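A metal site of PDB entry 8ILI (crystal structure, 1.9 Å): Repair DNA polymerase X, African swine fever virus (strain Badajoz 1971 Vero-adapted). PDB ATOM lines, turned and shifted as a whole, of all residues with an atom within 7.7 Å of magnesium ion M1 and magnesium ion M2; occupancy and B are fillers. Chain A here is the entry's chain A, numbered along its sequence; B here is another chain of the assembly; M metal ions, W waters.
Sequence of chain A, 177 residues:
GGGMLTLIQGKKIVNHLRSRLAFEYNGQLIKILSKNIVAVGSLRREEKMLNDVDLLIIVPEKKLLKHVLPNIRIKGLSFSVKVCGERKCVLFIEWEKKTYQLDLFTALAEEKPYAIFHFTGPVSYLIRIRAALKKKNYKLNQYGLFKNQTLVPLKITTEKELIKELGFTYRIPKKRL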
ATOM      1  N   VAL A  40     -21.740  -8.448  35.772  1.00  0.00           N
ATOM      2  CA  VAL A  40     -20.810  -8.825  34.696  1.00  0.00           C
ATOM      3  C   VAL A  40     -20.227  -7.545  34.082  1.00  0.00           C
ATOM      4  O   VAL A  40     -20.295  -6.468  34.695  1.00  0.00           O
ATOM      5  CB  VAL A  40     -21.476  -9.785  33.670  1.00  0.00           C
ATOM      6  CG1 VAL A  40     -21.807 -11.116  34.347  1.00  0.00           C
ATOM      7  CG2 VAL A  40     -22.739  -9.192  33.056  1.00  0.00           C
ATOM      8  N   GLY A  41     -19.603  -7.661  32.904  1.00  0.00           N
ATOM      9  CA  GLY A  41     -19.087  -6.498  32.193  1.00  0.00           C
ATOM     10  C   GLY A  41     -17.937  -5.813  32.925  1.00  0.00           C
ATOM     11  O   GLY A  41     -17.270  -6.411  33.779  1.00  0.00           O
ATOM     12  N   SER A  42     -17.728  -4.550  32.593  1.00  0.00           N
ATOM     13  CA  SER A  42     -16.628  -3.768  33.165  1.00  0.00           C
ATOM     14  C   SER A  42     -16.736  -3.604  34.688  1.00  0.00           C
ATOM     15  O   SER A  42     -15.722  -3.493  35.382  1.00  0.00           O
ATOM     16  CB  SER A  42     -16.511  -2.408  32.466  1.00  0.00           C
ATOM     17  OG  SER A  42     -17.642  -1.603  32.672  1.00  0.00           O
ATOM     18  N   LEU A  43     -17.972  -3.647  35.217  1.00  0.00           N
ATOM     19  CA  LEU A  43     -18.207  -3.646  36.660  1.00  0.00           C
ATOM     20  C   LEU A  43     -17.557  -4.846  37.342  1.00  0.00           C
ATOM     21  O   LEU A  43     -16.899  -4.687  38.373  1.00  0.00           O
ATOM     22  CB  LEU A  43     -19.707  -3.625  36.962  1.00  0.00           C
ATOM     23  CG  LEU A  43     -20.152  -3.573  38.432  1.00  0.00           C
ATOM     24  CD1 LEU A  43     -20.126  -2.167  38.978  1.00  0.00           C
ATOM     25  CD2 LEU A  43     -21.564  -4.115  38.572  1.00  0.00           C
ATOM     26  N   ARG A  45     -15.077  -6.549  36.083  1.00  0.00           N
ATOM     27  CA  ARG A  45     -13.641  -6.330  35.866  1.00  0.00           C
ATOM     28  C   ARG A  45     -13.040  -5.208  36.742  1.00  0.00           C
ATOM     29  O   ARG A  45     -11.839  -4.960  36.680  1.00  0.00           O
ATOM     30  CB  ARG A  45     -13.351  -6.051  34.394  1.00  0.00           C
ATOM     31  CG  ARG A  45     -13.732  -7.204  33.469  1.00  0.00           C
ATOM     32  CD  ARG A  45     -12.993  -7.107  32.137  1.00  0.00           C
ATOM     33  NE  ARG A  45     -13.180  -5.810  31.476  1.00  0.00           N
ATOM     34  CZ  ARG A  45     -14.262  -5.441  30.772  1.00  0.00           C
ATOM     35  NH1 ARG A  45     -15.300  -6.255  30.603  1.00  0.00           N
ATOM     36  NH2 ARG A  45     -14.289  -4.239  30.222  1.00  0.00           N
ATOM     37  N   LEU A  50     -17.262   3.307  34.331  1.00  0.00           N
ATOM     38  CA  LEU A  50     -18.127   2.383  33.614  1.00  0.00           C
ATOM     39  C   LEU A  50     -18.945   3.178  32.606  1.00  0.00           C
ATOM     40  O   LEU A  50     -19.379   4.273  32.901  1.00  0.00           O
ATOM     41  CB  LEU A  50     -19.075   1.667  34.586  1.00  0.00           C
ATOM     42  CG  LEU A  50     -18.472   1.051  35.857  1.00  0.00           C
ATOM     43  CD1 LEU A  50     -19.577   0.487  36.717  1.00  0.00           C
ATOM     44  CD2 LEU A  50     -17.450  -0.028  35.531  1.00  0.00           C
ATOM     45  N   ASN A  51     -19.112   2.611  31.419  1.00  0.00           N
ATOM     46  CA  ASN A  51     -20.031   3.165  30.427  1.00  0.00           C
ATOM     47  C   ASN A  51     -21.471   2.789  30.711  1.00  0.00           C
ATOM     48  O   ASN A  51     -22.379   3.414  30.182  1.00  0.00           O
ATOM     49  CB  ASN A  51     -19.650   2.701  29.015  1.00  0.00           C
ATOM     50  CG  ASN A  51     -18.406   3.394  28.483  1.00  0.00           C
ATOM     51  OD1 ASN A  51     -18.351   4.619  28.466  1.00  0.00           O
ATOM     52  ND2 ASN A  51     -17.425   2.627  28.044  1.00  0.00           N
ATOM     53  N   ASP A  52     -21.679   1.742  31.523  1.00  0.00           N
ATOM     54  CA  ASP A  52     -23.014   1.222  31.847  1.00  0.00           C
ATOM     55  C   ASP A  52     -22.900   0.134  32.919  1.00  0.00           C
ATOM     56  O   ASP A  52     -21.793  -0.252  33.285  1.00  0.00           O
ATOM     57  CB  ASP A  52     -23.667   0.657  30.593  1.00  0.00           C
ATOM     58  CG  ASP A  52     -22.763  -0.275  29.849  1.00  0.00           C
ATOM     59  OD1 ASP A  52     -22.561  -1.422  30.326  1.00  0.00           O
ATOM     60  OD2 ASP A  52     -22.218   0.125  28.791  1.00  0.00           O
ATOM     61  N   VAL A  53     -24.040  -0.344  33.397  1.00  0.00           N
ATOM     62  CA  VAL A  53     -24.095  -1.435  34.378  1.00  0.00           C
ATOM     63  C   VAL A  53     -24.615  -2.672  33.674  1.00  0.00           C
ATOM     64  O   VAL A  53     -25.651  -2.617  33.012  1.00  0.00           O
ATOM     65  CB  VAL A  53     -25.005  -1.085  35.566  1.00  0.00           C
ATOM     66  CG1 VAL A  53     -25.052  -2.228  36.588  1.00  0.00           C
ATOM     67  CG2 VAL A  53     -24.510   0.183  36.245  1.00  0.00           C
ATOM     68  N   ASP A  54     -23.876  -3.783  33.800  1.00  0.00           N
ATOM     69  CA  ASP A  54     -24.250  -5.062  33.178  1.00  0.00           C
ATOM     70  C   ASP A  54     -24.648  -6.104  34.214  1.00  0.00           C
ATOM     71  O   ASP A  54     -23.861  -6.423  35.110  1.00  0.00           O
ATOM     72  CB  ASP A  54     -23.079  -5.618  32.358  1.00  0.00           C
ATOM     73  CG  ASP A  54     -22.683  -4.724  31.224  1.00  0.00           C
ATOM     74  OD1 ASP A  54     -23.524  -4.436  30.348  1.00  0.00           O
ATOM     75  OD2 ASP A  54     -21.505  -4.312  31.177  1.00  0.00           O
ATOM     76  N   LEU A  55     -25.855  -6.634  34.079  1.00  0.00           N
ATOM     77  CA  LEU A  55     -26.337  -7.713  34.928  1.00  0.00           C
ATOM     78  C   LEU A  55     -26.720  -8.920  34.081  1.00  0.00           C
ATOM     79  O   LEU A  55     -27.368  -8.780  33.034  1.00  0.00           O
ATOM     80  CB  LEU A  55     -27.549  -7.275  35.749  1.00  0.00           C
ATOM     81  CG  LEU A  55     -27.325  -6.209  36.826  1.00  0.00           C
ATOM     82  CD1 LEU A  55     -28.631  -5.948  37.554  1.00  0.00           C
ATOM     83  CD2 LEU A  55     -26.239  -6.613  37.815  1.00  0.00           C
ATOM     84  N   VAL A  90     -31.755  -3.486  26.930  1.00  0.00           N
ATOM     85  CA  VAL A  90     -31.006  -2.284  27.311  1.00  0.00           C
ATOM     86  C   VAL A  90     -32.008  -1.269  27.860  1.00  0.00           C
ATOM     87  O   VAL A  90     -32.948  -0.883  27.148  1.00  0.00           O
ATOM     88  CB  VAL A  90     -30.255  -1.677  26.105  1.00  0.00           C
ATOM     89  CG1 VAL A  90     -29.496  -0.407  26.512  1.00  0.00           C
ATOM     90  CG2 VAL A  90     -29.295  -2.694  25.507  1.00  0.00           C
ATOM     91  N   GLN A 101     -27.239   3.820  31.597  1.00  0.00           N
ATOM     92  CA  GLN A 101     -27.626   2.650  30.827  1.00  0.00           C
ATOM     93  C   GLN A 101     -27.449   1.389  31.677  1.00  0.00           C
ATOM     94  O   GLN A 101     -26.390   1.187  32.298  1.00  0.00           O
ATOM     95  CB  GLN A 101     -26.803   2.559  29.542  1.00  0.00           C
ATOM     96  CG  GLN A 101     -27.126   1.346  28.674  1.00  0.00           C
ATOM     97  CD  GLN A 101     -26.512   1.398  27.287  1.00  0.00           C
ATOM     98  OE1 GLN A 101     -26.474   2.460  26.662  1.00  0.00           O
ATOM     99  NE2 GLN A 101     -26.048   0.260  26.791  1.00  0.00           N
ATOM    100  N   LEU A 102     -28.496   0.566  31.726  1.00  0.00           N
ATOM    101  CA  LEU A 102     -28.493  -0.723  32.401  1.00  0.00           C
ATOM    102  C   LEU A 102     -28.723  -1.802  31.338  1.00  0.00           C
ATOM    103  O   LEU A 102     -29.747  -1.803  30.671  1.00  0.00           O
ATOM    104  CB  LEU A 102     -29.605  -0.770  33.457  1.00  0.00           C
ATOM    105  CG  LEU A 102     -29.864  -2.086  34.209  1.00  0.00           C
ATOM    106  CD1 LEU A 102     -28.630  -2.548  34.977  1.00  0.00           C
ATOM    107  CD2 LEU A 102     -31.046  -1.930  35.151  1.00  0.00           C
ATOM    108  N   ASP A 103     -27.755  -2.705  31.198  1.00  0.00           N
ATOM    109  CA  ASP A 103     -27.845  -3.788  30.235  1.00  0.00           C
ATOM    110  C   ASP A 103     -28.134  -5.115  30.920  1.00  0.00           C
ATOM    111  O   ASP A 103     -27.335  -5.601  31.720  1.00  0.00           O
ATOM    112  CB  ASP A 103     -26.549  -3.889  29.423  1.00  0.00           C
ATOM    113  CG  ASP A 103     -26.332  -2.690  28.515  1.00  0.00           C
ATOM    114  OD1 ASP A 103     -27.331  -2.155  28.004  1.00  0.00           O
ATOM    115  OD2 ASP A 103     -25.161  -2.305  28.309  1.00  0.00           O
ATOM    116  N   LEU A 104     -29.291  -5.697  30.613  1.00  0.00           N
ATOM    117  CA  LEU A 104     -29.708  -6.960  31.201  1.00  0.00           C
ATOM    118  C   LEU A 104     -29.543  -8.067  30.169  1.00  0.00           C
ATOM    119  O   LEU A 104     -29.952  -7.914  29.008  1.00  0.00           O
ATOM    120  CB  LEU A 104     -31.170  -6.898  31.629  1.00  0.00           C
ATOM    121  CG  LEU A 104     -31.550  -5.762  32.580  1.00  0.00           C
ATOM    122  CD1 LEU A 104     -33.040  -5.820  32.868  1.00  0.00           C
ATOM    123  CD2 LEU A 104     -30.741  -5.836  33.875  1.00  0.00           C
ATOM    124  N   PHE A 105     -28.971  -9.175  30.600  1.00  0.00           N
ATOM    125  CA  PHE A 105     -28.804 -10.351  29.764  1.00  0.00           C
ATOM    126  C   PHE A 105     -29.343 -11.562  30.506  1.00  0.00           C
ATOM    127  O   PHE A 105     -29.323 -11.578  31.756  1.00  0.00           O
ATOM    128  CB  PHE A 105     -27.337 -10.567  29.408  1.00  0.00           C
ATOM    129  CG  PHE A 105     -26.663  -9.344  28.853  1.00  0.00           C
ATOM    130  CD1 PHE A 105     -26.805  -8.990  27.522  1.00  0.00           C
ATOM    131  CD2 PHE A 105     -25.855  -8.540  29.678  1.00  0.00           C
ATOM    132  CE1 PHE A 105     -26.174  -7.873  27.006  1.00  0.00           C
ATOM    133  CE2 PHE A 105     -25.228  -7.415  29.168  1.00  0.00           C
ATOM    134  CZ  PHE A 105     -25.386  -7.078  27.829  1.00  0.00           C
ATOM    135  N   PHE A 119     -19.785 -12.609  29.173  1.00  0.00           N
ATOM    136  CA  PHE A 119     -20.205 -11.261  29.598  1.00  0.00           C
ATOM    137  C   PHE A 119     -19.185 -10.526  30.480  1.00  0.00           C
ATOM    138  O   PHE A 119     -19.285  -9.320  30.652  1.00  0.00           O
ATOM    139  CB  PHE A 119     -21.595 -11.302  30.250  1.00  0.00           C
ATOM    140  CG  PHE A 119     -22.695 -11.550  29.259  1.00  0.00           C
ATOM    141  CD1 PHE A 119     -23.012 -10.578  28.305  1.00  0.00           C
ATOM    142  CD2 PHE A 119     -23.400 -12.753  29.242  1.00  0.00           C
ATOM    143  CE1 PHE A 119     -24.011 -10.796  27.372  1.00  0.00           C
ATOM    144  CE2 PHE A 119     -24.392 -12.972  28.297  1.00  0.00           C
ATOM    145  CZ  PHE A 119     -24.686 -12.003  27.366  1.00  0.00           C
ATOM    146  P    DC B   6     -24.243   2.223  17.438  1.00  0.00           P
ATOM    147  OP1  DC B   6     -24.933   3.393  18.053  1.00  0.00           O
ATOM    148  OP2  DC B   6     -22.859   2.342  16.957  1.00  0.00           O
ATOM    149  O5'  DC B   6     -24.328   1.048  18.513  1.00  0.00           O
ATOM    150  C5'  DC B   6     -25.603   0.630  19.047  1.00  0.00           C
ATOM    151  C4'  DC B   6     -25.494  -0.762  19.627  1.00  0.00           C
ATOM    152  O4'  DC B   6     -25.170  -1.701  18.579  1.00  0.00           O
ATOM    153  C3'  DC B   6     -24.391  -0.951  20.669  1.00  0.00           C
ATOM    154  O3'  DC B   6     -24.870  -0.735  21.992  1.00  0.00           O
ATOM    155  C2'  DC B   6     -24.007  -2.413  20.495  1.00  0.00           C
ATOM    156  C1'  DC B   6     -24.695  -2.870  19.212  1.00  0.00           C
ATOM    157  N1   DC B   6     -23.803  -3.596  18.296  1.00  0.00           N
ATOM    158  C2   DC B   6     -23.901  -4.989  18.251  1.00  0.00           C
ATOM    159  O2   DC B   6     -24.744  -5.557  18.962  1.00  0.00           O
ATOM    160  N3   DC B   6     -23.074  -5.673  17.433  1.00  0.00           N
ATOM    161  C4   DC B   6     -22.156  -5.029  16.711  1.00  0.00           C
ATOM    162  N4   DC B   6     -21.366  -5.756  15.908  1.00  0.00           N
ATOM    163  C5   DC B   6     -22.023  -3.612  16.751  1.00  0.00           C
ATOM    164  C6   DC B   6     -22.855  -2.938  17.558  1.00  0.00           C
ATOM    165  P    DC B   7     -23.869  -0.818  23.262  1.00  0.00           P
ATOM    166  OP1  DC B   7     -24.547  -0.147  24.407  1.00  0.00           O
ATOM    167  OP2  DC B   7     -22.511  -0.380  22.841  1.00  0.00           O
ATOM    168  O5'  DC B   7     -23.770  -2.384  23.544  1.00  0.00           O
ATOM    169  C5'  DC B   7     -24.893  -3.136  24.045  1.00  0.00           C
ATOM    170  C4'  DC B   7     -24.474  -4.559  24.342  1.00  0.00           C
ATOM    171  O4'  DC B   7     -24.508  -5.354  23.128  1.00  0.00           O
ATOM    172  C3'  DC B   7     -23.054  -4.757  24.863  1.00  0.00           C
ATOM    173  O3'  DC B   7     -22.856  -4.408  26.233  1.00  0.00           O
ATOM    174  C2'  DC B   7     -22.845  -6.239  24.595  1.00  0.00           C
ATOM    175  C1'  DC B   7     -23.543  -6.404  23.252  1.00  0.00           C
ATOM    176  N1   DC B   7     -22.624  -6.314  22.094  1.00  0.00           N
ATOM    177  C2   DC B   7     -22.057  -7.501  21.596  1.00  0.00           C
ATOM    178  O2   DC B   7     -22.374  -8.584  22.123  1.00  0.00           O
ATOM    179  N3   DC B   7     -21.195  -7.436  20.562  1.00  0.00           N
ATOM    180  C4   DC B   7     -20.887  -6.255  20.023  1.00  0.00           C
ATOM    181  N4   DC B   7     -20.033  -6.240  18.996  1.00  0.00           N
ATOM    182  C5   DC B   7     -21.414  -5.035  20.525  1.00  0.00           C
ATOM    183  C6   DC B   7     -22.275  -5.114  21.561  1.00  0.00           C
ATOM    184  P   GMS B   8     -21.395  -4.014  26.727  1.00  0.00           P
ATOM    185  OP1 GMS B   8     -21.539  -3.497  28.120  1.00  0.00           O
ATOM    186 SE   GMS B   8     -20.350  -3.024  25.478  1.00  0.00          SE
ATOM    187  O5' GMS B   8     -20.693  -5.431  26.879  1.00  0.00           O
ATOM    188  N9  GMS B   8     -19.084  -8.328  24.803  1.00  0.00           N
ATOM    189  C4  GMS B   8     -18.623  -9.013  23.694  1.00  0.00           C
ATOM    190  N3  GMS B   8     -18.365 -10.335  23.640  1.00  0.00           N
ATOM    191  C2  GMS B   8     -17.959 -10.707  22.442  1.00  0.00           C
ATOM    192  N2  GMS B   8     -17.658 -11.998  22.206  1.00  0.00           N
ATOM    193  N1  GMS B   8     -17.810  -9.839  21.378  1.00  0.00           N
ATOM    194  C6  GMS B   8     -18.076  -8.484  21.416  1.00  0.00           C
ATOM    195  O6  GMS B   8     -17.918  -7.795  20.403  1.00  0.00           O
ATOM    196  C5  GMS B   8     -18.514  -8.069  22.699  1.00  0.00           C
ATOM    197  N7  GMS B   8     -18.883  -6.813  23.161  1.00  0.00           N
ATOM    198  C8  GMS B   8     -19.187  -7.012  24.413  1.00  0.00           C
ATOM    199  C2' GMS B   8     -18.149  -8.550  27.083  1.00  0.00           C
ATOM    200  C5' GMS B   8     -21.028  -6.328  27.950  1.00  0.00           C
ATOM    201  C4' GMS B   8     -20.147  -7.560  27.865  1.00  0.00           C
ATOM    202  O4' GMS B   8     -20.470  -8.305  26.673  1.00  0.00           O
ATOM    203  C1' GMS B   8     -19.293  -8.890  26.130  1.00  0.00           C
ATOM    204  C3' GMS B   8     -18.639  -7.293  27.753  1.00  0.00           C
ATOM    205  O3' GMS B   8     -18.022  -7.080  29.020  1.00  0.00           O
HETATM  206 MG    MG M   1     -23.299  -2.973  28.897  1.00  0.00          MG
HETATM  207 MG    MG M   2     -20.706  -2.840  30.001  1.00  0.00          MG
HETATM  208  O   HOH W   1     -18.916  -3.883  30.031  1.00  0.00           O
HETATM  209  O   HOH W   2     -20.049  -0.944  28.297  1.00  0.00           O
HETATM  210  O   HOH W   3     -19.765  -2.098  32.097  1.00  0.00           O
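O of Val 53 sits at hydrogen-bond distance from N of Asp 103, at 2.8 Å. O of Asp 103 sits at hydrogen-bond distance from N of Leu 55 (3.0 Å). OP1 of DC 7 of chain B lies within hydrogen-bond range of NE2 of Gln 101, at 2.8 Å. The side-chain amide nitrogen of Gln 101 lies within hydrogen-bond range of the side-chain carboxylate of Asp 103, 3.0 Å away. O of Asp 54 lies within hydrogen-bond range of N of Val 40 (3.0 Å). NH1 of Arg 45 sits at hydrogen-bond distance from O3' of GMS 8 of chain B, 3.3 Å away.
O3' of DC 7 of chain B touches magnesium ion M1, 3.1 Å away. Within 4 Å of magnesium ion M1: Asp 52, Asp 54, Asp 103, DC 7 of chain B and GMS 8 of chain B. Along chain A the residues within 4 Å of magnesium ion M1 span positions 52 to 103.
Three residues have an atom within 4 Å of magnesium ion M2: Asp 52, Asp 54 and GMS 8 of chain B.
Magnesium ion M1 is bound by OP1 of GMS 8 of chain B (2.0 Å). OD2 of Asp 103 binds magnesium ion M1, at 2.1 Å. Magnesium ion M1 is bound by OD1 of Asp 54 (2.1 Å). OD1 of Asp 52 is bound to magnesium ion M1 (2.2 Å). Magnesium ion M1 has four donor atoms within binding distance.
Magnesium ion M2 is bound by OD2 of Asp 54 (2.0 Å), water W1 (2.1 Å), OP1 of GMS 8 of chain B (2.2 Å), OD1 of Asp 52 (2.4 Å) and water W3 (2.4 Å). Magnesium ion M2 has five donor atoms within binding distance. Slightly farther from magnesium ion M2 lies water W2 (2.6 Å).
Water W1 lies within hydrogen-bond range of N of Ser 42 (2.9 Å) and O3' of GMS 8 of chain B (3.5 Å). Water W3 lies within hydrogen-bond range of the backbone carbonyl oxygen (O) of Asp 52 (3.0 Å) and the backbone NH (N) of Ser 42 (3.2 Å).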
